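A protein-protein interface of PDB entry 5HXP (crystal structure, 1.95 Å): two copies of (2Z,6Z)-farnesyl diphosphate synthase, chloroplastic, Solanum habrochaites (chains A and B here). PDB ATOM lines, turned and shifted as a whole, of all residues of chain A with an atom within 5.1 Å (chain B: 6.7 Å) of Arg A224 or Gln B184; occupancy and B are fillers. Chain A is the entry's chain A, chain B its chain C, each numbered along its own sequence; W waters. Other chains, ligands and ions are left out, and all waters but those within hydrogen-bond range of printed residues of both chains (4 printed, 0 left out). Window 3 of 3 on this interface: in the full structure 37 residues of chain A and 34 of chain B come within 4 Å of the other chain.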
ATOM      1  N   THR A 197      15.297   7.718 -19.131  1.00  0.00           N
ATOM      2  CA  THR A 197      14.318   7.882 -18.071  1.00  0.00           C
ATOM      3  C   THR A 197      13.262   8.940 -18.387  1.00  0.00           C
ATOM      4  O   THR A 197      13.573   9.986 -18.925  1.00  0.00           O
ATOM      5  CB  THR A 197      15.033   8.241 -16.748  1.00  0.00           C
ATOM      6  OG1 THR A 197      15.981   7.210 -16.441  1.00  0.00           O
ATOM      7  CG2 THR A 197      14.036   8.375 -15.609  1.00  0.00           C
ATOM      8  N   GLU A 198      12.006   8.641 -18.070  1.00  0.00           N
ATOM      9  CA  GLU A 198      10.936   9.634 -18.097  1.00  0.00           C
ATOM     10  C   GLU A 198      11.047  10.572 -16.887  1.00  0.00           C
ATOM     11  O   GLU A 198      11.193  10.119 -15.772  1.00  0.00           O
ATOM     12  CB  GLU A 198       9.550   8.960 -18.079  1.00  0.00           C
ATOM     13  CG  GLU A 198       9.164   8.262 -19.360  1.00  0.00           C
ATOM     14  CD  GLU A 198       9.133   9.200 -20.548  1.00  0.00           C
ATOM     15  OE1 GLU A 198       8.759  10.396 -20.399  1.00  0.00           O
ATOM     16  OE2 GLU A 198       9.537   8.747 -21.634  1.00  0.00           O
ATOM     17  N   PHE A 199      10.946  11.877 -17.126  1.00  0.00           N
ATOM     18  CA  PHE A 199      11.033  12.883 -16.075  1.00  0.00           C
ATOM     19  C   PHE A 199       9.666  13.402 -15.666  1.00  0.00           C
ATOM     20  O   PHE A 199       8.833  13.710 -16.523  1.00  0.00           O
ATOM     21  CB  PHE A 199      11.842  14.097 -16.535  1.00  0.00           C
ATOM     22  CG  PHE A 199      13.271  13.804 -16.929  1.00  0.00           C
ATOM     23  CD1 PHE A 199      13.918  12.656 -16.547  1.00  0.00           C
ATOM     24  CD2 PHE A 199      13.977  14.735 -17.669  1.00  0.00           C
ATOM     25  CE1 PHE A 199      15.245  12.428 -16.912  1.00  0.00           C
ATOM     26  CE2 PHE A 199      15.296  14.509 -18.044  1.00  0.00           C
ATOM     27  CZ  PHE A 199      15.933  13.354 -17.649  1.00  0.00           C
ATOM     28  N   TYR A 200       9.452  13.528 -14.358  1.00  0.00           N
ATOM     29  CA  TYR A 200       8.235  14.132 -13.823  1.00  0.00           C
ATOM     30  C   TYR A 200       8.589  15.196 -12.778  1.00  0.00           C
ATOM     31  O   TYR A 200       9.245  14.892 -11.780  1.00  0.00           O
ATOM     32  CB  TYR A 200       7.350  13.041 -13.211  1.00  0.00           C
ATOM     33  CG  TYR A 200       6.074  13.570 -12.609  1.00  0.00           C
ATOM     34  CD1 TYR A 200       4.905  13.673 -13.375  1.00  0.00           C
ATOM     35  CD2 TYR A 200       6.034  13.979 -11.287  1.00  0.00           C
ATOM     36  CE1 TYR A 200       3.735  14.194 -12.822  1.00  0.00           C
ATOM     37  CE2 TYR A 200       4.874  14.487 -10.728  1.00  0.00           C
ATOM     38  CZ  TYR A 200       3.732  14.590 -11.491  1.00  0.00           C
ATOM     39  OH  TYR A 200       2.589  15.082 -10.910  1.00  0.00           O
ATOM     40  N   PHE A 201       8.148  16.433 -13.009  1.00  0.00           N
ATOM     41  CA  PHE A 201       8.476  17.564 -12.144  1.00  0.00           C
ATOM     42  C   PHE A 201       7.236  18.052 -11.449  1.00  0.00           C
ATOM     43  O   PHE A 201       6.176  18.189 -12.086  1.00  0.00           O
ATOM     44  CB  PHE A 201       9.071  18.706 -12.961  1.00  0.00           C
ATOM     45  CG  PHE A 201      10.341  18.332 -13.640  1.00  0.00           C
ATOM     46  CD1 PHE A 201      11.490  18.145 -12.902  1.00  0.00           C
ATOM     47  CD2 PHE A 201      10.368  18.078 -15.010  1.00  0.00           C
ATOM     48  CE1 PHE A 201      12.675  17.743 -13.513  1.00  0.00           C
ATOM     49  CE2 PHE A 201      11.552  17.675 -15.631  1.00  0.00           C
ATOM     50  CZ  PHE A 201      12.701  17.517 -14.890  1.00  0.00           C
ATOM     51  N   ASN A 220       0.715   9.665 -14.569  1.00  0.00           N
ATOM     52  CA  ASN A 220       1.264  10.470 -15.619  1.00  0.00           C
ATOM     53  C   ASN A 220       2.306   9.695 -16.434  1.00  0.00           C
ATOM     54  O   ASN A 220       2.294   9.753 -17.662  1.00  0.00           O
ATOM     55  CB  ASN A 220       1.835  11.757 -15.027  1.00  0.00           C
ATOM     56  CG  ASN A 220       2.349  12.706 -16.080  1.00  0.00           C
ATOM     57  OD1 ASN A 220       3.372  12.448 -16.715  1.00  0.00           O
ATOM     58  ND2 ASN A 220       1.656  13.830 -16.254  1.00  0.00           N
ATOM     59  N   PHE A 221       3.185   8.965 -15.748  1.00  0.00           N
ATOM     60  CA  PHE A 221       4.186   8.105 -16.395  1.00  0.00           C
ATOM     61  C   PHE A 221       3.532   7.093 -17.346  1.00  0.00           C
ATOM     62  O   PHE A 221       3.951   6.939 -18.497  1.00  0.00           O
ATOM     63  CB  PHE A 221       5.013   7.358 -15.324  1.00  0.00           C
ATOM     64  CG  PHE A 221       5.860   6.228 -15.861  1.00  0.00           C
ATOM     65  CD1 PHE A 221       7.032   6.487 -16.558  1.00  0.00           C
ATOM     66  CD2 PHE A 221       5.497   4.901 -15.657  1.00  0.00           C
ATOM     67  CE1 PHE A 221       7.815   5.452 -17.060  1.00  0.00           C
ATOM     68  CE2 PHE A 221       6.271   3.864 -16.157  1.00  0.00           C
ATOM     69  CZ  PHE A 221       7.444   4.133 -16.846  1.00  0.00           C
ATOM     70  N   GLN A 222       2.513   6.408 -16.844  1.00  0.00           N
ATOM     71  CA  GLN A 222       1.819   5.364 -17.611  1.00  0.00           C
ATOM     72  C   GLN A 222       1.188   5.901 -18.906  1.00  0.00           C
ATOM     73  O   GLN A 222       1.066   5.180 -19.876  1.00  0.00           O
ATOM     74  CB  GLN A 222       0.777   4.659 -16.726  1.00  0.00           C
ATOM     75  CG  GLN A 222       1.413   3.902 -15.569  1.00  0.00           C
ATOM     76  CD  GLN A 222       0.432   3.123 -14.724  1.00  0.00           C
ATOM     77  OE1 GLN A 222      -0.775   3.347 -14.784  1.00  0.00           O
ATOM     78  NE2 GLN A 222       0.947   2.202 -13.923  1.00  0.00           N
ATOM     79  N   GLN A 223       0.817   7.172 -18.931  1.00  0.00           N
ATOM     80  CA  GLN A 223       0.244   7.776 -20.138  1.00  0.00           C
ATOM     81  C   GLN A 223       1.261   8.050 -21.255  1.00  0.00           C
ATOM     82  O   GLN A 223       0.880   8.286 -22.401  1.00  0.00           O
ATOM     83  CB  GLN A 223      -0.480   9.073 -19.775  1.00  0.00           C
ATOM     84  CG  GLN A 223      -1.708   8.842 -18.905  1.00  0.00           C
ATOM     85  CD  GLN A 223      -2.318  10.133 -18.387  1.00  0.00           C
ATOM     86  OE1 GLN A 223      -1.877  11.236 -18.736  1.00  0.00           O
ATOM     87  NE2 GLN A 223      -3.335  10.004 -17.539  1.00  0.00           N
ATOM     88  N   ARG A 224       2.550   8.017 -20.935  1.00  0.00           N
ATOM     89  CA  ARG A 224       3.576   8.415 -21.897  1.00  0.00           C
ATOM     90  C   ARG A 224       4.061   7.280 -22.777  1.00  0.00           C
ATOM     91  O   ARG A 224       4.205   6.145 -22.309  1.00  0.00           O
ATOM     92  CB  ARG A 224       4.760   8.987 -21.154  1.00  0.00           C
ATOM     93  CG  ARG A 224       4.382  10.132 -20.246  1.00  0.00           C
ATOM     94  CD  ARG A 224       5.601  10.526 -19.473  1.00  0.00           C
ATOM     95  NE  ARG A 224       5.349  11.525 -18.447  1.00  0.00           N
ATOM     96  CZ  ARG A 224       6.319  12.224 -17.868  1.00  0.00           C
ATOM     97  NH1 ARG A 224       7.591  12.037 -18.238  1.00  0.00           N
ATOM     98  NH2 ARG A 224       6.016  13.113 -16.936  1.00  0.00           N
ATOM     99  N   HIS A 225       4.359   7.617 -24.032  1.00  0.00           N
ATOM    100  CA  HIS A 225       4.866   6.665 -25.033  1.00  0.00           C
ATOM    101  C   HIS A 225       6.396   6.720 -25.087  1.00  0.00           C
ATOM    102  O   HIS A 225       6.978   7.733 -25.502  1.00  0.00           O
ATOM    103  CB  HIS A 225       4.311   6.960 -26.438  1.00  0.00           C
ATOM    104  CG  HIS A 225       2.934   7.544 -26.441  1.00  0.00           C
ATOM    105  ND1 HIS A 225       1.803   6.792 -26.195  1.00  0.00           N
ATOM    106  CD2 HIS A 225       2.506   8.811 -26.652  1.00  0.00           C
ATOM    107  CE1 HIS A 225       0.739   7.573 -26.257  1.00  0.00           C
ATOM    108  NE2 HIS A 225       1.139   8.802 -26.532  1.00  0.00           N
ATOM    109  N   ARG A 226       7.027   5.617 -24.691  1.00  0.00           N
ATOM    110  CA  ARG A 226       8.482   5.499 -24.659  1.00  0.00           C
ATOM    111  C   ARG A 226       8.974   4.824 -25.939  1.00  0.00           C
ATOM    112  O   ARG A 226       8.580   3.698 -26.236  1.00  0.00           O
ATOM    113  CB  ARG A 226       8.902   4.695 -23.425  1.00  0.00           C
ATOM    114  CG  ARG A 226       8.419   5.312 -22.113  1.00  0.00           C
ATOM    115  CD  ARG A 226       8.958   4.581 -20.898  1.00  0.00           C
ATOM    116  NE  ARG A 226      10.388   4.810 -20.688  1.00  0.00           N
ATOM    117  CZ  ARG A 226      11.151   4.104 -19.848  1.00  0.00           C
ATOM    118  NH1 ARG A 226      12.444   4.391 -19.717  1.00  0.00           N
ATOM    119  NH2 ARG A 226      10.635   3.109 -19.129  1.00  0.00           N
ATOM    120  N   ARG B 179      13.382  20.904 -25.580  1.00  0.00           N
ATOM    121  CA  ARG B 179      12.898  19.764 -26.343  1.00  0.00           C
ATOM    122  C   ARG B 179      11.465  19.955 -26.850  1.00  0.00           C
ATOM    123  O   ARG B 179      10.529  20.124 -26.068  1.00  0.00           O
ATOM    124  CB  ARG B 179      12.960  18.488 -25.529  1.00  0.00           C
ATOM    125  CG  ARG B 179      12.412  17.293 -26.277  1.00  0.00           C
ATOM    126  CD  ARG B 179      12.813  15.985 -25.649  1.00  0.00           C
ATOM    127  NE  ARG B 179      12.345  14.883 -26.484  1.00  0.00           N
ATOM    128  CZ  ARG B 179      12.863  13.664 -26.496  1.00  0.00           C
ATOM    129  NH1 ARG B 179      13.901  13.347 -25.713  1.00  0.00           N
ATOM    130  NH2 ARG B 179      12.351  12.756 -27.322  1.00  0.00           N
ATOM    131  N   GLY B 182       6.877  17.406 -26.912  1.00  0.00           N
ATOM    132  CA  GLY B 182       6.139  17.043 -25.696  1.00  0.00           C
ATOM    133  C   GLY B 182       6.659  15.923 -24.794  1.00  0.00           C
ATOM    134  O   GLY B 182       6.154  15.756 -23.687  1.00  0.00           O
ATOM    135  N   ASP B 183       7.652  15.161 -25.240  1.00  0.00           N
ATOM    136  CA  ASP B 183       8.180  14.048 -24.439  1.00  0.00           C
ATOM    137  C   ASP B 183       9.204  14.581 -23.434  1.00  0.00           C
ATOM    138  O   ASP B 183       9.965  15.489 -23.750  1.00  0.00           O
ATOM    139  CB  ASP B 183       8.807  12.993 -25.333  1.00  0.00           C
ATOM    140  CG  ASP B 183       7.921  12.644 -26.519  1.00  0.00           C
ATOM    141  OD1 ASP B 183       6.943  11.914 -26.307  1.00  0.00           O
ATOM    142  OD2 ASP B 183       8.199  13.098 -27.651  1.00  0.00           O
ATOM    143  N   GLN B 184       9.196  14.023 -22.228  1.00  0.00           N
ATOM    144  CA  GLN B 184       9.950  14.602 -21.100  1.00  0.00           C
ATOM    145  C   GLN B 184      11.080  13.651 -20.724  1.00  0.00           C
ATOM    146  O   GLN B 184      10.972  12.863 -19.795  1.00  0.00           O
ATOM    147  CB  GLN B 184       9.029  14.897 -19.926  1.00  0.00           C
ATOM    148  CG  GLN B 184       8.143  16.113 -20.137  1.00  0.00           C
ATOM    149  CD  GLN B 184       7.211  16.362 -18.973  1.00  0.00           C
ATOM    150  OE1 GLN B 184       6.075  15.893 -18.961  1.00  0.00           O
ATOM    151  NE2 GLN B 184       7.697  17.047 -17.974  1.00  0.00           N
ATOM    152  N   ARG B 185      12.135  13.729 -21.519  1.00  0.00           N
ATOM    153  CA  ARG B 185      13.285  12.844 -21.444  1.00  0.00           C
ATOM    154  C   ARG B 185      14.424  13.491 -22.226  1.00  0.00           C
ATOM    155  O   ARG B 185      14.191  14.423 -23.012  1.00  0.00           O
ATOM    156  CB  ARG B 185      12.940  11.467 -22.007  1.00  0.00           C
ATOM    157  CG  ARG B 185      12.061  11.502 -23.254  1.00  0.00           C
ATOM    158  CD  ARG B 185      11.965  10.112 -23.857  1.00  0.00           C
ATOM    159  NE  ARG B 185      11.082  10.025 -25.031  1.00  0.00           N
ATOM    160  CZ  ARG B 185       9.767   9.777 -24.999  1.00  0.00           C
ATOM    161  NH1 ARG B 185       9.103   9.669 -23.858  1.00  0.00           N
ATOM    162  NH2 ARG B 185       9.096   9.662 -26.142  1.00  0.00           N
ATOM    163  N   VAL B 186      15.655  13.026 -22.004  1.00  0.00           N
ATOM    164  CA  VAL B 186      16.820  13.549 -22.730  1.00  0.00           C
ATOM    165  C   VAL B 186      17.306  12.584 -23.838  1.00  0.00           C
ATOM    166  O   VAL B 186      18.131  12.952 -24.662  1.00  0.00           O
ATOM    167  CB  VAL B 186      18.008  13.953 -21.783  1.00  0.00           C
ATOM    168  CG1 VAL B 186      17.636  15.125 -20.886  1.00  0.00           C
ATOM    169  CG2 VAL B 186      18.490  12.796 -20.941  1.00  0.00           C
ATOM    170  N   PHE B 201      10.434  21.745 -21.735  1.00  0.00           N
ATOM    171  CA  PHE B 201       9.789  20.781 -22.597  1.00  0.00           C
ATOM    172  C   PHE B 201       8.522  21.435 -23.128  1.00  0.00           C
ATOM    173  O   PHE B 201       7.757  21.999 -22.345  1.00  0.00           O
ATOM    174  CB  PHE B 201       9.470  19.526 -21.808  1.00  0.00           C
ATOM    175  CG  PHE B 201      10.683  18.801 -21.285  1.00  0.00           C
ATOM    176  CD1 PHE B 201      11.480  18.046 -22.137  1.00  0.00           C
ATOM    177  CD2 PHE B 201      11.006  18.835 -19.928  1.00  0.00           C
ATOM    178  CE1 PHE B 201      12.581  17.342 -21.660  1.00  0.00           C
ATOM    179  CE2 PHE B 201      12.102  18.134 -19.443  1.00  0.00           C
ATOM    180  CZ  PHE B 201      12.892  17.383 -20.313  1.00  0.00           C
HETATM  181  O   HOH W   1       6.458  17.056 -15.472  1.00  0.00           O
HETATM  182  O   HOH W   2       7.424  11.892 -22.038  1.00  0.00           O
HETATM  183  O   HOH W   3       3.993  16.035 -16.523  1.00  0.00           O
HETATM  184  O   HOH W   4      15.746  10.634 -20.373  1.00  0.00           O
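Printed residues of chain B within 4 Å of Arg A224: Gln B184. Printed residues of chain A within 4 Å of Gln B184: Thr A197 (3.97 Å), Glu A198 (3.4 Å), Phe A199 (2.8 Å) and Arg A224 (3.4 Å). Of the printed residues of chain A, Arg B185 touches Thr A197 (3.5 Å), Glu A198 (2.4 Å) and His A225 (2.9 Å). Of the printed residues of chain B, Glu A198 touches Gln B184 (3.4 Å) and Arg B185 (2.4 Å). Of the printed residues of chain A, Phe B201 touches Phe A199 (3.9 Å) and Phe A201 (3.9 Å). Printed residues of chain A within 4 Å of Val B186: Phe A199 (3.7 Å). The nearest residue of chain A that does not touch Gln B184 is Phe A201 (4.1 Å). The nearest printed residue of chain B that does not touch Glu A198 is Asp B183 (5.2 Å).
OE1 of Glu A198 is in salt-bridge range of NH1 of Arg A224, 3.0 Å away. NH1 of Arg A224 lies within hydrogen-bond range of O of Phe A199, at 2.7 Å. NH2 of Arg A224 sits at hydrogen-bond distance from OD1 of Asn A220 (2.7 Å). NH1 of Arg B179 sits at hydrogen-bond distance from O of Arg B185 (2.9 Å). OD1 of Asp B183 lies within salt-bridge range of NH2 of Arg B185 (3.1 Å).
Water W2 lies within hydrogen-bond range of OE1 of Glu A198, N of Gln B184 and NH1 of Arg B185. Water W4 lies within hydrogen-bond range of the backbone carbonyl oxygen (O) of Thr A197 (2.7 Å) and the backbone NH (N) of Val B186 (2.9 Å). Water W1 lies within hydrogen-bond range of NE2 of Gln B184 and N of Phe A201. Water W3 lies within hydrogen-bond range of the side-chain amide oxygen (OE1) of Gln B184 (3.2 Å) and the side-chain amide nitrogen (ND2) of Asn A220 (3.2 Å).
OE2 of Glu A198 lies within salt-bridge range of NH1 of Arg B185 (2.4 Å). The backbone carbonyl oxygen (O) of Gln B184 sits at hydrogen-bond distance from the backbone NH (N) of Phe A199. OE1 of Gln B184 lies within hydrogen-bond range of NH2 of Arg A224 (3.4 Å). The backbone carbonyl oxygen (O) of His A225 is in hydrogen-bond range of the guanidinium group (NH2) of Arg B185, at 2.9 Å. The side-chain carboxylate (OE1) of Glu A198 sits close to the backbone carbonyl oxygen (O) of Gln B184 (3.4 Å).
Thr A197 touches Gln B184 (O to O, 3.97 Å). Arg B185 touches Thr A197. CE2 of Phe A199 touches CG1 of Val B186, at 3.7 Å. CD2 of Phe A199 touches CZ of Phe B201, at 3.9 Å. Phe A201 touches Phe B201 (CE2 to CE2, 3.9 Å).
Hydrophobic or aromatic side chains of chain B within 4 Å of the printed part of chain A: Val B186 and Phe B201. Hydrophobic or aromatic side chains of chain A within 4 Å of the printed part of chain B: Phe A199 and Phe A201. Among the printed residues, 10 pairs touch across the chains. Among the printed residues, Asp or Glu carboxylates within 4 Å of a Lys or Arg side-chain nitrogen of the other chain: Glu A198 with Arg B185.
Phe A201 touches its own counterpart, Phe B201. Position printed for both chains: 201.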
